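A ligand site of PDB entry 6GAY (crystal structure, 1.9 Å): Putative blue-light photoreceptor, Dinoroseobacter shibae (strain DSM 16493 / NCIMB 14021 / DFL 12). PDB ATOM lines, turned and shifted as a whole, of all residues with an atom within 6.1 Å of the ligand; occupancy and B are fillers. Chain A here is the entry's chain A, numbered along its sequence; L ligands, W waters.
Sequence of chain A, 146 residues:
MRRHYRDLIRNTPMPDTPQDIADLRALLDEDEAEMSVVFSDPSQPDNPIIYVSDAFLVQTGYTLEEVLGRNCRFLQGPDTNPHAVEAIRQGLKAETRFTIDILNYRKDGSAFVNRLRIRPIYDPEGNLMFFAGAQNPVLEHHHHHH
The side-chain amide nitrogen of Asn 114 is in hydrogen-bond range of an oxygen (O2) of the ligand, at 3.1 Å.
An oxygen (O8) of the ligand is in salt-bridge range of the guanidinium group of Arg 73 (3.0 Å).
The side-chain amide oxygen (OD1) of Asn 71 lies within hydrogen-bond range of an oxygen (O3) of the ligand (2.7 Å).
The side-chain amide nitrogen (NE2) of Gln 135 is in hydrogen-bond range of an oxygen (O2) of the ligand (2.9 Å).
NE2 of Gln 76 lies within hydrogen-bond range of O1 of the ligand (2.9 Å).
A nitrogen (N2) of the ligand sits at hydrogen-bond distance from the side-chain amide oxygen of Asn 104.
The side-chain sulfur (SG) of Cys 72 is in hydrogen-bond range of a nitrogen (N3) of the ligand (3.5 Å).
The guanidinium group of Arg 89 is in salt-bridge range of the side-chain carboxylate of Glu 86 (2.9 Å).
The side-chain amide nitrogen (ND2) of Asn 71 is in hydrogen-bond range of the backbone carbonyl oxygen (O) of Asp 46, 3.0 Å away.
N of Arg 73 sits at hydrogen-bond distance from OD1 of Asn 71 (2.7 Å).
The side-chain amide oxygen of Asn 114 sits close to the backbone NH of Leu 116 (3.4 Å).
The backbone NH (N) of Asn 114 lies within hydrogen-bond range of the backbone carbonyl oxygen (O) of Ile 102 (2.8 Å).
O of Phe 131 lies within hydrogen-bond range of N of Ser 40 (2.8 Å).
NH1 of Arg 73 is in salt-bridge range of OD2 of Asp 46 (2.7 Å).
The side-chain amide nitrogen (ND2) of Asn 47 lies within hydrogen-bond range of the side-chain hydroxyl (OG) of Ser 40 (2.7 Å).
Val 38 touches the ligand (CG2 to C5, 3.6 Å).
Ser 40 touches the ligand.
Leu 75 touches the ligand (CD1 to O2, 3.4 Å).
O of Val 85 touches C17 of the ligand, 3.5 Å away.
CG2 of Ile 88 touches C13 of the ligand, 3.7 Å away.
Arg 89 touches the ligand.
CD1 of Leu 92 touches O4 of the ligand, at 3.3 Å.
Ile 102 touches the ligand.
CD1 of Leu 116 touches N3 of the ligand, 3.4 Å away.
Ile 118 touches the ligand.
Phe 131 touches the ligand (O to C7, 3.5 Å).
C of Ala 132 touches C7 of the ligand (3.7 Å).
N of Gly 133 touches C7 of the ligand, at 3.5 Å.
Within 4 Å of the ligand: Val 38, Ser 40, Asn 71, Cys 72, Arg 73, Leu 75, Gln 76, Val 85, Ile 88, Arg 89, Leu 92, Ile 102, Asn 104, Asn 114, Leu 116, Ile 118, Phe 131, Ala 132, Gly 133 and Gln 135.
The nearest printed residue that does not touch the ligand is Asn 47 (4.01 Å).
Water W2 bridges the side-chain amide nitrogen (ND2) of Asn 71 and an oxygen (O4) of the ligand.
Water W4 lies within hydrogen-bond range of OE1 of Gln 76 (2.6 Å) and O8 of the ligand (2.8 Å).
Water W3 lies within hydrogen-bond range of O of Asn 47 (3.0 Å), N of Cys 72 (3.0 Å), O3 of the ligand (3.1 Å) and ND2 of Asn 71 (3.4 Å).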
ATOM      1  N   VAL A  38      15.001 -17.256 -12.774  1.00  0.00           N
ATOM      2  CA  VAL A  38      14.019 -16.263 -13.186  1.00  0.00           C
ATOM      3  C   VAL A  38      14.005 -15.155 -12.141  1.00  0.00           C
ATOM      4  O   VAL A  38      14.350 -15.375 -10.975  1.00  0.00           O
ATOM      5  CB  VAL A  38      12.594 -16.844 -13.371  1.00  0.00           C
ATOM      6  CG1 VAL A  38      12.625 -18.046 -14.373  1.00  0.00           C
ATOM      7  CG2 VAL A  38      11.990 -17.277 -12.047  1.00  0.00           C
ATOM      8  N   PHE A  39      13.636 -13.966 -12.568  1.00  0.00           N
ATOM      9  CA  PHE A  39      13.309 -12.842 -11.696  1.00  0.00           C
ATOM     10  C   PHE A  39      11.816 -12.568 -11.885  1.00  0.00           C
ATOM     11  O   PHE A  39      11.318 -12.493 -13.028  1.00  0.00           O
ATOM     12  CB  PHE A  39      14.114 -11.573 -12.026  1.00  0.00           C
ATOM     13  CG  PHE A  39      15.599 -11.661 -11.708  1.00  0.00           C
ATOM     14  CD1 PHE A  39      16.386 -12.655 -12.240  1.00  0.00           C
ATOM     15  CD2 PHE A  39      16.174 -10.719 -10.908  1.00  0.00           C
ATOM     16  CE1 PHE A  39      17.732 -12.728 -11.918  1.00  0.00           C
ATOM     17  CE2 PHE A  39      17.534 -10.746 -10.611  1.00  0.00           C
ATOM     18  CZ  PHE A  39      18.288 -11.777 -11.119  1.00  0.00           C
ATOM     19  N   SER A  40      11.138 -12.311 -10.778  1.00  0.00           N
ATOM     20  CA  SER A  40       9.749 -11.919 -10.736  1.00  0.00           C
ATOM     21  C   SER A  40       9.579 -10.490 -10.168  1.00  0.00           C
ATOM     22  O   SER A  40      10.462  -9.924  -9.524  1.00  0.00           O
ATOM     23  CB  SER A  40       8.955 -12.891  -9.887  1.00  0.00           C
ATOM     24  OG  SER A  40       9.337 -12.722  -8.475  1.00  0.00           O
ATOM     25  N   ASP A  46       0.491 -11.279  -8.514  1.00  0.00           N
ATOM     26  CA  ASP A  46       0.876 -12.661  -8.467  1.00  0.00           C
ATOM     27  C   ASP A  46       2.347 -12.863  -8.872  1.00  0.00           C
ATOM     28  O   ASP A  46       2.665 -13.906  -9.441  1.00  0.00           O
ATOM     29  CB  ASP A  46      -0.027 -13.493  -9.371  1.00  0.00           C
ATOM     30  CG  ASP A  46       0.064 -14.947  -9.062  1.00  0.00           C
ATOM     31  OD1 ASP A  46       0.252 -15.209  -7.866  1.00  0.00           O
ATOM     32  OD2 ASP A  46      -0.100 -15.829  -9.989  1.00  0.00           O
ATOM     33  N   ASN A  47       3.231 -11.884  -8.691  1.00  0.00           N
ATOM     34  CA  ASN A  47       4.670 -12.093  -8.783  1.00  0.00           C
ATOM     35  C   ASN A  47       5.056 -12.711 -10.128  1.00  0.00           C
ATOM     36  O   ASN A  47       5.662 -13.777 -10.172  1.00  0.00           O
ATOM     37  CB  ASN A  47       5.125 -13.027  -7.669  1.00  0.00           C
ATOM     38  CG  ASN A  47       6.262 -12.478  -6.824  1.00  0.00           C
ATOM     39  OD1 ASN A  47       6.339 -12.788  -5.656  1.00  0.00           O
ATOM     40  ND2 ASN A  47       7.106 -11.693  -7.387  1.00  0.00           N
ATOM     41  N   PHE A  56      17.154 -21.570 -18.164  1.00  0.00           N
ATOM     42  CA  PHE A  56      15.799 -21.919 -17.730  1.00  0.00           C
ATOM     43  C   PHE A  56      14.993 -22.553 -18.857  1.00  0.00           C
ATOM     44  O   PHE A  56      14.339 -23.610 -18.668  1.00  0.00           O
ATOM     45  CB  PHE A  56      15.106 -20.666 -17.176  1.00  0.00           C
ATOM     46  CG  PHE A  56      13.703 -20.892 -16.658  1.00  0.00           C
ATOM     47  CD1 PHE A  56      12.616 -20.918 -17.534  1.00  0.00           C
ATOM     48  CD2 PHE A  56      13.480 -21.213 -15.326  1.00  0.00           C
ATOM     49  CE1 PHE A  56      11.332 -21.166 -17.079  1.00  0.00           C
ATOM     50  CE2 PHE A  56      12.214 -21.450 -14.892  1.00  0.00           C
ATOM     51  CZ  PHE A  56      11.127 -21.412 -15.796  1.00  0.00           C
ATOM     52  N   ASN A  71       3.329 -16.492 -13.281  1.00  0.00           N
ATOM     53  CA  ASN A  71       3.932 -17.018 -12.061  1.00  0.00           C
ATOM     54  C   ASN A  71       4.621 -18.361 -12.311  1.00  0.00           C
ATOM     55  O   ASN A  71       4.127 -19.206 -13.091  1.00  0.00           O
ATOM     56  CB  ASN A  71       2.837 -17.165 -11.028  1.00  0.00           C
ATOM     57  CG  ASN A  71       3.351 -17.621  -9.678  1.00  0.00           C
ATOM     58  OD1 ASN A  71       3.628 -18.811  -9.495  1.00  0.00           O
ATOM     59  ND2 ASN A  71       3.409 -16.666  -8.673  1.00  0.00           N
ATOM     60  N   CYS A  72       5.741 -18.595 -11.614  1.00  0.00           N
ATOM     61  CA  CYS A  72       6.503 -19.800 -11.909  1.00  0.00           C
ATOM     62  C   CYS A  72       5.840 -21.088 -11.401  1.00  0.00           C
ATOM     63  O   CYS A  72       6.390 -22.168 -11.647  1.00  0.00           O
ATOM     64  CB  CYS A  72       7.916 -19.684 -11.295  1.00  0.00           C
ATOM     65  SG  CYS A  72       9.174 -20.542 -12.323  1.00  0.00           S
ATOM     66  N   ARG A  73       4.670 -21.023 -10.739  1.00  0.00           N
ATOM     67  CA  ARG A  73       4.075 -22.269 -10.254  1.00  0.00           C
ATOM     68  C   ARG A  73       3.657 -23.267 -11.365  1.00  0.00           C
ATOM     69  O   ARG A  73       3.210 -24.381 -11.053  1.00  0.00           O
ATOM     70  CB  ARG A  73       2.840 -21.981  -9.389  1.00  0.00           C
ATOM     71  CG  ARG A  73       1.638 -21.412 -10.189  1.00  0.00           C
ATOM     72  CD  ARG A  73       0.420 -21.350  -9.256  1.00  0.00           C
ATOM     73  NE  ARG A  73       0.656 -20.346  -8.211  1.00  0.00           N
ATOM     74  CZ  ARG A  73       0.502 -19.034  -8.354  1.00  0.00           C
ATOM     75  NH1 ARG A  73       0.116 -18.509  -9.497  1.00  0.00           N
ATOM     76  NH2 ARG A  73       0.740 -18.215  -7.347  1.00  0.00           N
ATOM     77  N   LEU A  75       5.585 -24.793 -13.067  1.00  0.00           N
ATOM     78  CA  LEU A  75       6.513 -25.926 -12.953  1.00  0.00           C
ATOM     79  C   LEU A  75       5.980 -27.010 -12.022  1.00  0.00           C
ATOM     80  O   LEU A  75       6.499 -28.125 -11.992  1.00  0.00           O
ATOM     81  CB  LEU A  75       7.881 -25.475 -12.472  1.00  0.00           C
ATOM     82  CG  LEU A  75       8.573 -24.539 -13.511  1.00  0.00           C
ATOM     83  CD1 LEU A  75       9.934 -24.021 -12.958  1.00  0.00           C
ATOM     84  CD2 LEU A  75       8.786 -25.267 -14.908  1.00  0.00           C
ATOM     85  N   GLN A  76       4.942 -26.733 -11.281  1.00  0.00           N
ATOM     86  CA  GLN A  76       4.454 -27.726 -10.339  1.00  0.00           C
ATOM     87  C   GLN A  76       3.523 -28.714 -11.044  1.00  0.00           C
ATOM     88  O   GLN A  76       3.041 -28.441 -12.150  1.00  0.00           O
ATOM     89  CB  GLN A  76       3.716 -27.018  -9.187  1.00  0.00           C
ATOM     90  CG  GLN A  76       4.768 -26.256  -8.340  1.00  0.00           C
ATOM     91  CD  GLN A  76       4.157 -25.197  -7.419  1.00  0.00           C
ATOM     92  OE1 GLN A  76       2.916 -25.155  -7.209  1.00  0.00           O
ATOM     93  NE2 GLN A  76       5.028 -24.280  -6.928  1.00  0.00           N
ATOM     94  N   THR A  80       3.657 -32.766  -6.651  1.00  0.00           N
ATOM     95  CA  THR A  80       4.241 -31.695  -5.866  1.00  0.00           C
ATOM     96  C   THR A  80       3.630 -31.652  -4.439  1.00  0.00           C
ATOM     97  O   THR A  80       2.420 -31.751  -4.242  1.00  0.00           O
ATOM     98  CB  THR A  80       4.017 -30.388  -6.615  1.00  0.00           C
ATOM     99  OG1 THR A  80       4.612 -30.492  -7.945  1.00  0.00           O
ATOM    100  CG2 THR A  80       4.608 -29.203  -5.773  1.00  0.00           C
ATOM    101  N   VAL A  85       4.822 -26.214  -1.270  1.00  0.00           N
ATOM    102  CA  VAL A  85       4.219 -25.044  -1.923  1.00  0.00           C
ATOM    103  C   VAL A  85       3.891 -23.980  -0.882  1.00  0.00           C
ATOM    104  O   VAL A  85       4.204 -22.773  -1.059  1.00  0.00           O
ATOM    105  CB  VAL A  85       2.973 -25.467  -2.736  1.00  0.00           C
ATOM    106  CG1 VAL A  85       2.168 -24.220  -3.203  1.00  0.00           C
ATOM    107  CG2 VAL A  85       3.336 -26.368  -3.886  1.00  0.00           C
ATOM    108  N   GLU A  86       3.338 -24.388   0.279  1.00  0.00           N
ATOM    109  CA  GLU A  86       2.981 -23.376   1.234  1.00  0.00           C
ATOM    110  C   GLU A  86       4.218 -22.817   1.899  1.00  0.00           C
ATOM    111  O   GLU A  86       4.215 -21.652   2.263  1.00  0.00           O
ATOM    112  CB  GLU A  86       1.984 -23.931   2.289  1.00  0.00           C
ATOM    113  CG  GLU A  86       1.627 -22.980   3.402  1.00  0.00           C
ATOM    114  CD  GLU A  86       0.753 -21.819   2.964  1.00  0.00           C
ATOM    115  OE1 GLU A  86       0.229 -21.888   1.817  1.00  0.00           O
ATOM    116  OE2 GLU A  86       0.585 -20.837   3.777  1.00  0.00           O
ATOM    117  N   ILE A  88       7.049 -22.119   0.430  1.00  0.00           N
ATOM    118  CA  ILE A  88       7.487 -21.040  -0.473  1.00  0.00           C
ATOM    119  C   ILE A  88       6.631 -19.801  -0.306  1.00  0.00           C
ATOM    120  O   ILE A  88       7.147 -18.662  -0.257  1.00  0.00           O
ATOM    121  CB  ILE A  88       7.429 -21.514  -1.939  1.00  0.00           C
ATOM    122  CG1 ILE A  88       8.363 -22.721  -2.178  1.00  0.00           C
ATOM    123  CG2 ILE A  88       7.796 -20.311  -2.859  1.00  0.00           C
ATOM    124  CD1 ILE A  88       8.030 -23.439  -3.543  1.00  0.00           C
ATOM    125  N   ARG A  89       5.307 -19.987  -0.304  1.00  0.00           N
ATOM    126  CA  ARG A  89       4.411 -18.856  -0.175  1.00  0.00           C
ATOM    127  C   ARG A  89       4.739 -18.078   1.091  1.00  0.00           C
ATOM    128  O   ARG A  89       4.775 -16.837   1.074  1.00  0.00           O
ATOM    129  CB  ARG A  89       2.957 -19.367  -0.147  1.00  0.00           C
ATOM    130  CG  ARG A  89       1.879 -18.301  -0.339  1.00  0.00           C
ATOM    131  CD  ARG A  89       0.485 -18.889  -0.542  1.00  0.00           C
ATOM    132  NE  ARG A  89      -0.073 -19.168   0.755  1.00  0.00           N
ATOM    133  CZ  ARG A  89      -0.669 -18.246   1.512  1.00  0.00           C
ATOM    134  NH1 ARG A  89      -0.799 -16.992   1.044  1.00  0.00           N
ATOM    135  NH2 ARG A  89      -1.136 -18.556   2.744  1.00  0.00           N
ATOM    136  N   LEU A  92       8.251 -16.252   0.776  1.00  0.00           N
ATOM    137  CA  LEU A  92       8.089 -15.001   0.015  1.00  0.00           C
ATOM    138  C   LEU A  92       7.453 -13.933   0.895  1.00  0.00           C
ATOM    139  O   LEU A  92       7.887 -12.774   0.849  1.00  0.00           O
ATOM    140  CB  LEU A  92       7.223 -15.212  -1.235  1.00  0.00           C
ATOM    141  CG  LEU A  92       7.888 -16.057  -2.322  1.00  0.00           C
ATOM    142  CD1 LEU A  92       6.847 -16.322  -3.420  1.00  0.00           C
ATOM    143  CD2 LEU A  92       9.025 -15.281  -2.956  1.00  0.00           C
ATOM    144  N   ILE A 102      11.649 -29.201  -4.098  1.00  0.00           N
ATOM    145  CA  ILE A 102      10.237 -29.311  -4.450  1.00  0.00           C
ATOM    146  C   ILE A 102      10.166 -30.038  -5.806  1.00  0.00           C
ATOM    147  O   ILE A 102      10.994 -29.798  -6.716  1.00  0.00           O
ATOM    148  CB  ILE A 102       9.552 -27.921  -4.478  1.00  0.00           C
ATOM    149  CG1 ILE A 102       8.069 -28.066  -4.858  1.00  0.00           C
ATOM    150  CG2 ILE A 102      10.225 -26.881  -5.479  1.00  0.00           C
ATOM    151  CD1 ILE A 102       7.323 -26.757  -4.776  1.00  0.00           C
ATOM    152  N   LEU A 103       9.213 -30.942  -5.927  1.00  0.00           N
ATOM    153  CA  LEU A 103       9.113 -31.688  -7.190  1.00  0.00           C
ATOM    154  C   LEU A 103       8.518 -30.799  -8.233  1.00  0.00           C
ATOM    155  O   LEU A 103       7.437 -30.208  -8.024  1.00  0.00           O
ATOM    156  CB  LEU A 103       8.228 -32.924  -7.038  1.00  0.00           C
ATOM    157  CG  LEU A 103       8.198 -33.900  -8.221  1.00  0.00           C
ATOM    158  CD1 LEU A 103       9.533 -34.625  -8.264  1.00  0.00           C
ATOM    159  CD2 LEU A 103       7.100 -34.916  -7.970  1.00  0.00           C
ATOM    160  N   ASN A 104       9.175 -30.750  -9.418  1.00  0.00           N
ATOM    161  CA  ASN A 104       8.653 -29.947 -10.508  1.00  0.00           C
ATOM    162  C   ASN A 104       8.606 -30.832 -11.753  1.00  0.00           C
ATOM    163  O   ASN A 104       9.127 -31.952 -11.763  1.00  0.00           O
ATOM    164  CB  ASN A 104       9.565 -28.729 -10.809  1.00  0.00           C
ATOM    165  CG  ASN A 104       9.387 -27.536  -9.840  1.00  0.00           C
ATOM    166  OD1 ASN A 104      10.080 -26.530 -10.000  1.00  0.00           O
ATOM    167  ND2 ASN A 104       8.393 -27.592  -8.946  1.00  0.00           N
ATOM    168  N   ASN A 114      13.535 -30.099  -7.732  1.00  0.00           N
ATOM    169  CA  ASN A 114      14.163 -28.810  -7.969  1.00  0.00           C
ATOM    170  C   ASN A 114      14.623 -28.248  -6.622  1.00  0.00           C
ATOM    171  O   ASN A 114      13.791 -28.092  -5.729  1.00  0.00           O
ATOM    172  CB  ASN A 114      13.118 -27.899  -8.624  1.00  0.00           C
ATOM    173  CG  ASN A 114      13.620 -26.433  -8.857  1.00  0.00           C
ATOM    174  OD1 ASN A 114      14.752 -26.088  -8.582  1.00  0.00           O
ATOM    175  ND2 ASN A 114      12.669 -25.555  -9.254  1.00  0.00           N
ATOM    176  N   LEU A 116      15.139 -25.225  -5.268  1.00  0.00           N
ATOM    177  CA  LEU A 116      14.784 -23.874  -5.684  1.00  0.00           C
ATOM    178  C   LEU A 116      15.334 -22.875  -4.679  1.00  0.00           C
ATOM    179  O   LEU A 116      15.025 -22.986  -3.476  1.00  0.00           O
ATOM    180  CB  LEU A 116      13.264 -23.740  -5.736  1.00  0.00           C
ATOM    181  CG  LEU A 116      12.660 -22.326  -5.784  1.00  0.00           C
ATOM    182  CD1 LEU A 116      13.032 -21.736  -7.164  1.00  0.00           C
ATOM    183  CD2 LEU A 116      11.158 -22.557  -5.681  1.00  0.00           C
ATOM    184  N   ILE A 118      15.535 -19.048  -3.603  1.00  0.00           N
ATOM    185  CA  ILE A 118      14.889 -17.757  -3.859  1.00  0.00           C
ATOM    186  C   ILE A 118      15.559 -16.698  -2.979  1.00  0.00           C
ATOM    187  O   ILE A 118      15.963 -17.007  -1.831  1.00  0.00           O
ATOM    188  CB  ILE A 118      13.373 -17.875  -3.599  1.00  0.00           C
ATOM    189  CG1 ILE A 118      12.662 -18.529  -4.781  1.00  0.00           C
ATOM    190  CG2 ILE A 118      12.765 -16.503  -3.219  1.00  0.00           C
ATOM    191  CD1 ILE A 118      11.312 -19.030  -4.369  1.00  0.00           C
ATOM    192  N   PHE A 131      12.169 -10.569  -6.916  1.00  0.00           N
ATOM    193  CA  PHE A 131      12.641 -11.816  -6.338  1.00  0.00           C
ATOM    194  C   PHE A 131      13.386 -12.546  -7.446  1.00  0.00           C
ATOM    195  O   PHE A 131      12.965 -12.478  -8.606  1.00  0.00           O
ATOM    196  CB  PHE A 131      11.478 -12.724  -5.901  1.00  0.00           C
ATOM    197  CG  PHE A 131      10.887 -12.250  -4.565  1.00  0.00           C
ATOM    198  CD1 PHE A 131      11.536 -12.623  -3.382  1.00  0.00           C
ATOM    199  CD2 PHE A 131       9.768 -11.502  -4.548  1.00  0.00           C
ATOM    200  CE1 PHE A 131      11.077 -12.189  -2.108  1.00  0.00           C
ATOM    201  CE2 PHE A 131       9.224 -11.038  -3.290  1.00  0.00           C
ATOM    202  CZ  PHE A 131       9.916 -11.407  -2.076  1.00  0.00           C
ATOM    203  N   ALA A 132      14.495 -13.204  -7.091  1.00  0.00           N
ATOM    204  CA  ALA A 132      15.176 -14.119  -8.008  1.00  0.00           C
ATOM    205  C   ALA A 132      14.957 -15.533  -7.522  1.00  0.00           C
ATOM    206  O   ALA A 132      14.988 -15.771  -6.323  1.00  0.00           O
ATOM    207  CB  ALA A 132      16.696 -13.852  -8.115  1.00  0.00           C
ATOM    208  N   GLY A 133      14.821 -16.496  -8.458  1.00  0.00           N
ATOM    209  CA  GLY A 133      14.542 -17.868  -8.069  1.00  0.00           C
ATOM    210  C   GLY A 133      15.322 -18.766  -9.005  1.00  0.00           C
ATOM    211  O   GLY A 133      15.028 -18.744 -10.206  1.00  0.00           O
ATOM    212  N   ALA A 134      16.337 -19.475  -8.506  1.00  0.00           N
ATOM    213  CA  ALA A 134      17.239 -20.288  -9.327  1.00  0.00           C
ATOM    214  C   ALA A 134      16.816 -21.750  -9.204  1.00  0.00           C
ATOM    215  O   ALA A 134      16.568 -22.227  -8.086  1.00  0.00           O
ATOM    216  CB  ALA A 134      18.703 -20.082  -8.895  1.00  0.00           C
ATOM    217  N   GLN A 135      16.681 -22.453 -10.333  1.00  0.00           N
ATOM    218  CA  GLN A 135      16.254 -23.840 -10.380  1.00  0.00           C
ATOM    219  C   GLN A 135      17.514 -24.699 -10.449  1.00  0.00           C
ATOM    220  O   GLN A 135      18.446 -24.432 -11.239  1.00  0.00           O
ATOM    221  CB  GLN A 135      15.392 -24.131 -11.610  1.00  0.00           C
ATOM    222  CG  GLN A 135      14.060 -23.371 -11.652  1.00  0.00           C
ATOM    223  CD  GLN A 135      14.214 -21.842 -11.781  1.00  0.00           C
ATOM    224  OE1 GLN A 135      15.104 -21.355 -12.508  1.00  0.00           O
ATOM    225  NE2 GLN A 135      13.300 -21.087 -11.144  1.00  0.00           N
HETATM  226  N1  LIG L   1       7.908 -22.676  -7.680  1.00  0.00           N
HETATM  227  C1  LIG L   1       8.293 -23.921  -8.243  1.00  0.00           C
HETATM  228  O1  LIG L   1       7.620 -24.896  -8.015  1.00  0.00           O
HETATM  229  N2  LIG L   1       9.419 -23.993  -9.077  1.00  0.00           N
HETATM  230  C2  LIG L   1      10.208 -22.876  -9.319  1.00  0.00           C
HETATM  231  O2  LIG L   1      11.267 -22.877 -10.012  1.00  0.00           O
HETATM  232  C3  LIG L   1       9.776 -21.626  -8.828  1.00  0.00           C
HETATM  233  N3  LIG L   1      10.556 -20.482  -9.073  1.00  0.00           N
HETATM  234  C4  LIG L   1      10.189 -19.269  -8.505  1.00  0.00           C
HETATM  235  C5  LIG L   1      10.946 -18.120  -8.712  1.00  0.00           C
HETATM  236  C6  LIG L   1      10.592 -16.924  -8.141  1.00  0.00           C
HETATM  237  C7  LIG L   1      11.378 -15.639  -8.414  1.00  0.00           C
HETATM  238  C8  LIG L   1       9.462 -16.817  -7.322  1.00  0.00           C
HETATM  239  C9  LIG L   1       9.053 -15.543  -6.702  1.00  0.00           C
HETATM  240  C10 LIG L   1       8.697 -17.963  -7.126  1.00  0.00           C
HETATM  241  C11 LIG L   1       9.076 -19.191  -7.662  1.00  0.00           C
HETATM  242  N4  LIG L   1       8.314 -20.342  -7.405  1.00  0.00           N
HETATM  243  C12 LIG L   1       8.655 -21.569  -8.002  1.00  0.00           C
HETATM  244  C13 LIG L   1       7.113 -20.355  -6.452  1.00  0.00           C
HETATM  245  C14 LIG L   1       5.734 -20.077  -7.021  1.00  0.00           C
HETATM  246  O3  LIG L   1       5.886 -19.013  -7.941  1.00  0.00           O
HETATM  247  C15 LIG L   1       4.751 -19.733  -5.904  1.00  0.00           C
HETATM  248  O4  LIG L   1       5.341 -18.639  -5.191  1.00  0.00           O
HETATM  249  C16 LIG L   1       4.490 -20.893  -4.925  1.00  0.00           C
HETATM  250  O5  LIG L   1       3.842 -21.906  -5.679  1.00  0.00           O
HETATM  251  C17 LIG L   1       3.668 -20.514  -3.666  1.00  0.00           C
HETATM  252  O6  LIG L   1       2.605 -19.703  -4.179  1.00  0.00           O
HETATM  253  P1  LIG L   1       1.158 -20.306  -4.240  1.00  0.00           P
HETATM  254  O7  LIG L   1       0.294 -19.126  -4.560  1.00  0.00           O
HETATM  255  O8  LIG L   1       1.344 -21.240  -5.482  1.00  0.00           O
HETATM  256  O9  LIG L   1       0.651 -21.080  -3.014  1.00  0.00           O
HETATM  257  O   HOH W   1       3.395 -17.069  -3.908  1.00  0.00           O
HETATM  258  O   HOH W   2       5.411 -16.357  -6.805  1.00  0.00           O
HETATM  259  O   HOH W   3       6.643 -16.519  -9.691  1.00  0.00           O
HETATM  260  O   HOH W   4       0.801 -23.854  -6.403  1.00  0.00           O
